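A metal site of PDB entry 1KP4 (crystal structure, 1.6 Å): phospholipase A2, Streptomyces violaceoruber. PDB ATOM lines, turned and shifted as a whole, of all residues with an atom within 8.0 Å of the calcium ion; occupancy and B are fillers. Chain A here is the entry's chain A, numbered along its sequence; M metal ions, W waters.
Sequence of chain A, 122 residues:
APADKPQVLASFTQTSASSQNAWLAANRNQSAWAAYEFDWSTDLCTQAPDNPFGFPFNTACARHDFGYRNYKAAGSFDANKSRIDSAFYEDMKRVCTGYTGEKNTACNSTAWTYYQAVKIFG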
ATOM      1  N   SER A  41      -6.959  18.860  -1.742  1.00  0.00           N
ATOM      2  CA  SER A  41      -7.699  18.283  -0.630  1.00  0.00           C
ATOM      3  C   SER A  41      -9.205  18.436  -0.787  1.00  0.00           C
ATOM      4  O   SER A  41      -9.648  19.386  -1.436  1.00  0.00           O
ATOM      5  CB  SER A  41      -7.290  18.992   0.661  1.00  0.00           C
ATOM      6  OG  SER A  41      -7.607  20.365   0.567  1.00  0.00           O
ATOM      7  N   THR A  42      -9.964  17.546  -0.184  1.00  0.00           N
ATOM      8  CA  THR A  42     -11.428  17.722  -0.219  1.00  0.00           C
ATOM      9  C   THR A  42     -12.102  17.096   1.002  1.00  0.00           C
ATOM     10  O   THR A  42     -11.640  16.054   1.468  1.00  0.00           O
ATOM     11  CB  THR A  42     -11.967  17.088  -1.511  1.00  0.00           C
ATOM     12  OG1 THR A  42     -13.405  17.048  -1.471  1.00  0.00           O
ATOM     13  CG2 THR A  42     -11.501  15.644  -1.626  1.00  0.00           C
ATOM     14  N   ASP A  43     -13.188  17.680   1.513  1.00  0.00           N
ATOM     15  CA  ASP A  43     -13.960  16.982   2.565  1.00  0.00           C
ATOM     16  C   ASP A  43     -15.266  16.429   1.972  1.00  0.00           C
ATOM     17  O   ASP A  43     -16.260  16.215   2.664  1.00  0.00           O
ATOM     18  CB  ASP A  43     -14.253  17.862   3.777  1.00  0.00           C
ATOM     19  CG  ASP A  43     -14.994  19.140   3.413  1.00  0.00           C
ATOM     20  OD1 ASP A  43     -15.121  20.049   4.266  1.00  0.00           O
ATOM     21  OD2 ASP A  43     -15.403  19.217   2.223  1.00  0.00           O
ATOM     22  N   LEU A  44     -15.247  16.192   0.659  1.00  0.00           N
ATOM     23  CA  LEU A  44     -16.423  15.652  -0.059  1.00  0.00           C
ATOM     24  C   LEU A  44     -17.616  16.544   0.240  1.00  0.00           C
ATOM     25  O   LEU A  44     -17.344  17.763   0.252  1.00  0.00           O
ATOM     26  CB  LEU A  44     -16.599  14.190   0.288  1.00  0.00           C
ATOM     27  CG  LEU A  44     -15.341  13.331   0.028  1.00  0.00           C
ATOM     28  CD1 LEU A  44     -15.666  11.860   0.222  1.00  0.00           C
ATOM     29  CD2 LEU A  44     -14.827  13.589  -1.385  1.00  0.00           C
ATOM     30  N   CYS A  45     -18.787  15.979   0.492  1.00  0.00           N
ATOM     31  CA  CYS A  45     -20.029  16.774   0.699  1.00  0.00           C
ATOM     32  C   CYS A  45     -20.277  17.030   2.174  1.00  0.00           C
ATOM     33  O   CYS A  45     -21.394  17.281   2.600  1.00  0.00           O
ATOM     34  CB  CYS A  45     -21.246  16.077   0.062  1.00  0.00           C
ATOM     35  SG  CYS A  45     -21.028  15.630  -1.689  1.00  0.00           S
ATOM     36  N   THR A  46     -19.227  16.981   3.000  1.00  0.00           N
ATOM     37  CA  THR A  46     -19.416  17.335   4.421  1.00  0.00           C
ATOM     38  C   THR A  46     -20.042  18.714   4.580  1.00  0.00           C
ATOM     39  O   THR A  46     -19.582  19.686   3.978  1.00  0.00           O
ATOM     40  CB  THR A  46     -18.062  17.312   5.159  1.00  0.00           C
ATOM     41  OG1 THR A  46     -17.498  16.004   4.945  1.00  0.00           O
ATOM     42  CG2 THR A  46     -18.233  17.522   6.662  1.00  0.00           C
ATOM     43  N   GLN A  47     -21.063  18.787   5.413  1.00  0.00           N
ATOM     44  CA  GLN A  47     -21.809  19.982   5.746  1.00  0.00           C
ATOM     45  C   GLN A  47     -22.786  20.399   4.656  1.00  0.00           C
ATOM     46  O   GLN A  47     -23.296  21.513   4.668  1.00  0.00           O
ATOM     47  CB  GLN A  47     -20.886  21.173   6.081  1.00  0.00           C
ATOM     48  CG  GLN A  47     -20.072  20.980   7.356  1.00  0.00           C
ATOM     49  CD  GLN A  47     -20.852  20.567   8.575  1.00  0.00           C
ATOM     50  OE1 GLN A  47     -21.314  21.406   9.352  1.00  0.00           O
ATOM     51  NE2 GLN A  47     -21.014  19.261   8.810  1.00  0.00           N
ATOM     52  N   ALA A  48     -23.084  19.498   3.722  1.00  0.00           N
ATOM     53  CA  ALA A  48     -24.111  19.722   2.717  1.00  0.00           C
ATOM     54  C   ALA A  48     -25.491  19.397   3.278  1.00  0.00           C
ATOM     55  O   ALA A  48     -25.563  18.824   4.364  1.00  0.00           O
ATOM     56  CB  ALA A  48     -23.844  18.855   1.502  1.00  0.00           C
ATOM     57  N   ASN A  58     -20.401  12.560  -4.293  1.00  0.00           N
ATOM     58  CA  ASN A  58     -19.068  12.847  -3.762  1.00  0.00           C
ATOM     59  C   ASN A  58     -18.123  13.421  -4.822  1.00  0.00           C
ATOM     60  O   ASN A  58     -17.354  14.347  -4.530  1.00  0.00           O
ATOM     61  CB  ASN A  58     -18.386  11.601  -3.161  1.00  0.00           C
ATOM     62  CG  ASN A  58     -18.970  11.303  -1.780  1.00  0.00           C
ATOM     63  OD1 ASN A  58     -19.620  12.181  -1.235  1.00  0.00           O
ATOM     64  ND2 ASN A  58     -18.720  10.125  -1.234  1.00  0.00           N
ATOM     65  N   ALA A  60     -18.778  15.231  -7.534  1.00  0.00           N
ATOM     66  CA  ALA A  60     -19.100  16.643  -7.699  1.00  0.00           C
ATOM     67  C   ALA A  60     -18.624  17.527  -6.561  1.00  0.00           C
ATOM     68  O   ALA A  60     -18.082  18.607  -6.848  1.00  0.00           O
ATOM     69  CB  ALA A  60     -20.612  16.834  -7.792  1.00  0.00           C
ATOM     70  N   CYS A  61     -18.806  17.115  -5.307  1.00  0.00           N
ATOM     71  CA  CYS A  61     -18.324  17.893  -4.163  1.00  0.00           C
ATOM     72  C   CYS A  61     -16.799  18.067  -4.220  1.00  0.00           C
ATOM     73  O   CYS A  61     -16.244  19.118  -3.881  1.00  0.00           O
ATOM     74  CB  CYS A  61     -18.739  17.225  -2.852  1.00  0.00           C
ATOM     75  SG  CYS A  61     -20.558  17.338  -2.638  1.00  0.00           S
ATOM     76  N   ALA A  62     -16.120  17.019  -4.673  1.00  0.00           N
ATOM     77  CA  ALA A  62     -14.653  17.102  -4.729  1.00  0.00           C
ATOM     78  C   ALA A  62     -14.184  18.166  -5.702  1.00  0.00           C
ATOM     79  O   ALA A  62     -13.226  18.911  -5.390  1.00  0.00           O
ATOM     80  CB  ALA A  62     -14.075  15.738  -5.080  1.00  0.00           C
ATOM     81  N   ARG A  63     -14.798  18.254  -6.893  1.00  0.00           N
ATOM     82  CA  ARG A  63     -14.313  19.233  -7.863  1.00  0.00           C
ATOM     83  C   ARG A  63     -14.725  20.615  -7.402  1.00  0.00           C
ATOM     84  O   ARG A  63     -13.995  21.581  -7.603  1.00  0.00           O
ATOM     85  CB  ARG A  63     -14.807  18.955  -9.295  1.00  0.00           C
ATOM     86  CG  ARG A  63     -14.224  19.924 -10.341  1.00  0.00           C
ATOM     87  CD  ARG A  63     -14.430  19.408 -11.751  1.00  0.00           C
ATOM     88  NE  ARG A  63     -15.751  19.718 -12.327  1.00  0.00           N
ATOM     89  CZ  ARG A  63     -15.966  20.626 -13.280  1.00  0.00           C
ATOM     90  NH1 ARG A  63     -14.982  21.373 -13.820  1.00  0.00           N
ATOM     91  NH2 ARG A  63     -17.217  20.786 -13.706  1.00  0.00           N
ATOM     92  N   HIS A  64     -15.877  20.703  -6.718  1.00  0.00           N
ATOM     93  CA  HIS A  64     -16.234  21.982  -6.115  1.00  0.00           C
ATOM     94  C   HIS A  64     -15.220  22.412  -5.055  1.00  0.00           C
ATOM     95  O   HIS A  64     -14.812  23.574  -5.022  1.00  0.00           O
ATOM     96  CB  HIS A  64     -17.665  21.899  -5.589  1.00  0.00           C
ATOM     97  CG  HIS A  64     -18.216  23.177  -5.066  1.00  0.00           C
ATOM     98  ND1 HIS A  64     -18.332  23.419  -3.711  1.00  0.00           N
ATOM     99  CD2 HIS A  64     -18.719  24.277  -5.694  1.00  0.00           C
ATOM    100  CE1 HIS A  64     -18.867  24.611  -3.519  1.00  0.00           C
ATOM    101  NE2 HIS A  64     -19.114  25.149  -4.697  1.00  0.00           N
ATOM    102  N   ASP A  65     -14.753  21.547  -4.161  1.00  0.00           N
ATOM    103  CA  ASP A  65     -13.682  21.935  -3.214  1.00  0.00           C
ATOM    104  C   ASP A  65     -12.439  22.353  -3.972  1.00  0.00           C
ATOM    105  O   ASP A  65     -11.761  23.317  -3.620  1.00  0.00           O
ATOM    106  CB  ASP A  65     -13.366  20.771  -2.257  1.00  0.00           C
ATOM    107  CG  ASP A  65     -14.442  20.532  -1.233  1.00  0.00           C
ATOM    108  OD1 ASP A  65     -14.666  19.377  -0.825  1.00  0.00           O
ATOM    109  OD2 ASP A  65     -15.084  21.466  -0.748  1.00  0.00           O
ATOM    110  N   PHE A  66     -12.110  21.654  -5.064  1.00  0.00           N
ATOM    111  CA  PHE A  66     -10.937  22.087  -5.833  1.00  0.00           C
ATOM    112  C   PHE A  66     -11.070  23.524  -6.303  1.00  0.00           C
ATOM    113  O   PHE A  66     -10.110  24.322  -6.192  1.00  0.00           O
ATOM    114  CB  PHE A  66     -10.703  21.110  -6.992  1.00  0.00           C
ATOM    115  CG  PHE A  66      -9.444  21.379  -7.796  1.00  0.00           C
ATOM    116  CD1 PHE A  66      -9.483  22.221  -8.894  1.00  0.00           C
ATOM    117  CD2 PHE A  66      -8.249  20.787  -7.428  1.00  0.00           C
ATOM    118  CE1 PHE A  66      -8.333  22.479  -9.619  1.00  0.00           C
ATOM    119  CE2 PHE A  66      -7.088  21.016  -8.160  1.00  0.00           C
ATOM    120  CZ  PHE A  66      -7.148  21.862  -9.266  1.00  0.00           C
ATOM    121  N   TYR A  68     -13.020  26.071  -5.081  1.00  0.00           N
ATOM    122  CA  TYR A  68     -12.963  26.964  -3.930  1.00  0.00           C
ATOM    123  C   TYR A  68     -11.542  27.080  -3.351  1.00  0.00           C
ATOM    124  O   TYR A  68     -11.070  28.182  -3.100  1.00  0.00           O
ATOM    125  CB  TYR A  68     -13.882  26.494  -2.815  1.00  0.00           C
ATOM    126  CG  TYR A  68     -15.312  26.955  -2.887  1.00  0.00           C
ATOM    127  CD1 TYR A  68     -16.029  27.250  -1.728  1.00  0.00           C
ATOM    128  CD2 TYR A  68     -15.945  27.115  -4.107  1.00  0.00           C
ATOM    129  CE1 TYR A  68     -17.350  27.687  -1.821  1.00  0.00           C
ATOM    130  CE2 TYR A  68     -17.277  27.542  -4.216  1.00  0.00           C
ATOM    131  CZ  TYR A  68     -17.960  27.826  -3.049  1.00  0.00           C
ATOM    132  OH  TYR A  68     -19.269  28.250  -3.103  1.00  0.00           O
ATOM    133  N   ARG A  69     -10.899  25.936  -3.077  1.00  0.00           N
ATOM    134  CA  ARG A  69      -9.634  26.031  -2.321  1.00  0.00           C
ATOM    135  C   ARG A  69      -8.557  26.678  -3.175  1.00  0.00           C
ATOM    136  O   ARG A  69      -7.773  27.502  -2.673  1.00  0.00           O
ATOM    137  CB  ARG A  69      -9.227  24.637  -1.821  1.00  0.00           C
ATOM    138  CG  ARG A  69     -10.211  24.170  -0.739  1.00  0.00           C
ATOM    139  CD  ARG A  69     -10.035  22.731  -0.308  1.00  0.00           C
ATOM    140  NE  ARG A  69     -11.178  22.310   0.520  1.00  0.00           N
ATOM    141  CZ  ARG A  69     -11.181  21.366   1.450  1.00  0.00           C
ATOM    142  NH1 ARG A  69     -10.093  20.673   1.735  1.00  0.00           N
ATOM    143  NH2 ARG A  69     -12.317  21.109   2.124  1.00  0.00           N
ATOM    144  N   PHE A  88     -20.560  22.920 -10.261  1.00  0.00           N
ATOM    145  CA  PHE A  88     -21.016  21.964  -9.252  1.00  0.00           C
ATOM    146  C   PHE A  88     -22.408  21.432  -9.572  1.00  0.00           C
ATOM    147  O   PHE A  88     -22.679  20.239  -9.558  1.00  0.00           O
ATOM    148  CB  PHE A  88     -21.015  22.621  -7.880  1.00  0.00           C
ATOM    149  CG  PHE A  88     -21.397  21.773  -6.679  1.00  0.00           C
ATOM    150  CD1 PHE A  88     -21.123  20.414  -6.566  1.00  0.00           C
ATOM    151  CD2 PHE A  88     -22.054  22.395  -5.621  1.00  0.00           C
ATOM    152  CE1 PHE A  88     -21.499  19.700  -5.426  1.00  0.00           C
ATOM    153  CE2 PHE A  88     -22.454  21.676  -4.500  1.00  0.00           C
ATOM    154  CZ  PHE A  88     -22.172  20.319  -4.380  1.00  0.00           C
ATOM    155  N   VAL A 118     -24.749  26.101  -1.551  1.00  0.00           N
ATOM    156  CA  VAL A 118     -23.423  26.724  -1.704  1.00  0.00           C
ATOM    157  C   VAL A 118     -23.550  28.131  -2.274  1.00  0.00           C
ATOM    158  O   VAL A 118     -22.709  29.001  -2.011  1.00  0.00           O
ATOM    159  CB  VAL A 118     -22.444  25.928  -2.585  1.00  0.00           C
ATOM    160  CG1 VAL A 118     -22.255  24.517  -2.029  1.00  0.00           C
ATOM    161  CG2 VAL A 118     -22.895  25.908  -4.043  1.00  0.00           C
HETATM  162 CA    CA M   1     -16.760  19.993   0.397  1.00  0.00          CA
HETATM  163  O   HOH W   1     -19.001  20.179   1.210  1.00  0.00           O
HETATM  164  O   HOH W   2     -16.777  22.171   1.445  1.00  0.00           O
HETATM  165  O   HOH W   3     -17.615  20.333  -1.734  1.00  0.00           O
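Three residues have an atom within 4 Å of the calcium ion: Asp 43, Leu 44 and Asp 65.
The nearest printed residue that does not touch the calcium ion is Cys 61 (4.4 Å).
The side-chain carboxylate of Asp 43 lies within salt-bridge range of the guanidinium group of Arg 69 (3.7 Å).
The side-chain hydroxyl of Thr 46 sits at hydrogen-bond distance from the backbone carbonyl oxygen of Asp 43 (2.6 Å).
OD1 of Asp 65 lies close to OG1 of Thr 42 (2.7 Å).
The side-chain sulfur (SG) of Cys 45 forms a disulfide with the side-chain sulfur (SG) of Cys 61.
OG1 of Thr 42 lies within hydrogen-bond range of N of Leu 44, 2.9 Å away.
The calcium ion is bound by the backbone carbonyl oxygen (O) of Leu 44 (2.3 Å), water W3 (2.3 Å), water W1 (2.4 Å), the side-chain carboxylate (OD2) of Asp 43 (2.4 Å), water W2 (2.4 Å), the side-chain carboxylate (OD1) of Asp 65 (2.5 Å) and the side-chain carboxylate (OD2) of Asp 65 (2.5 Å).
The calcium ion has seven donor atoms within binding distance.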
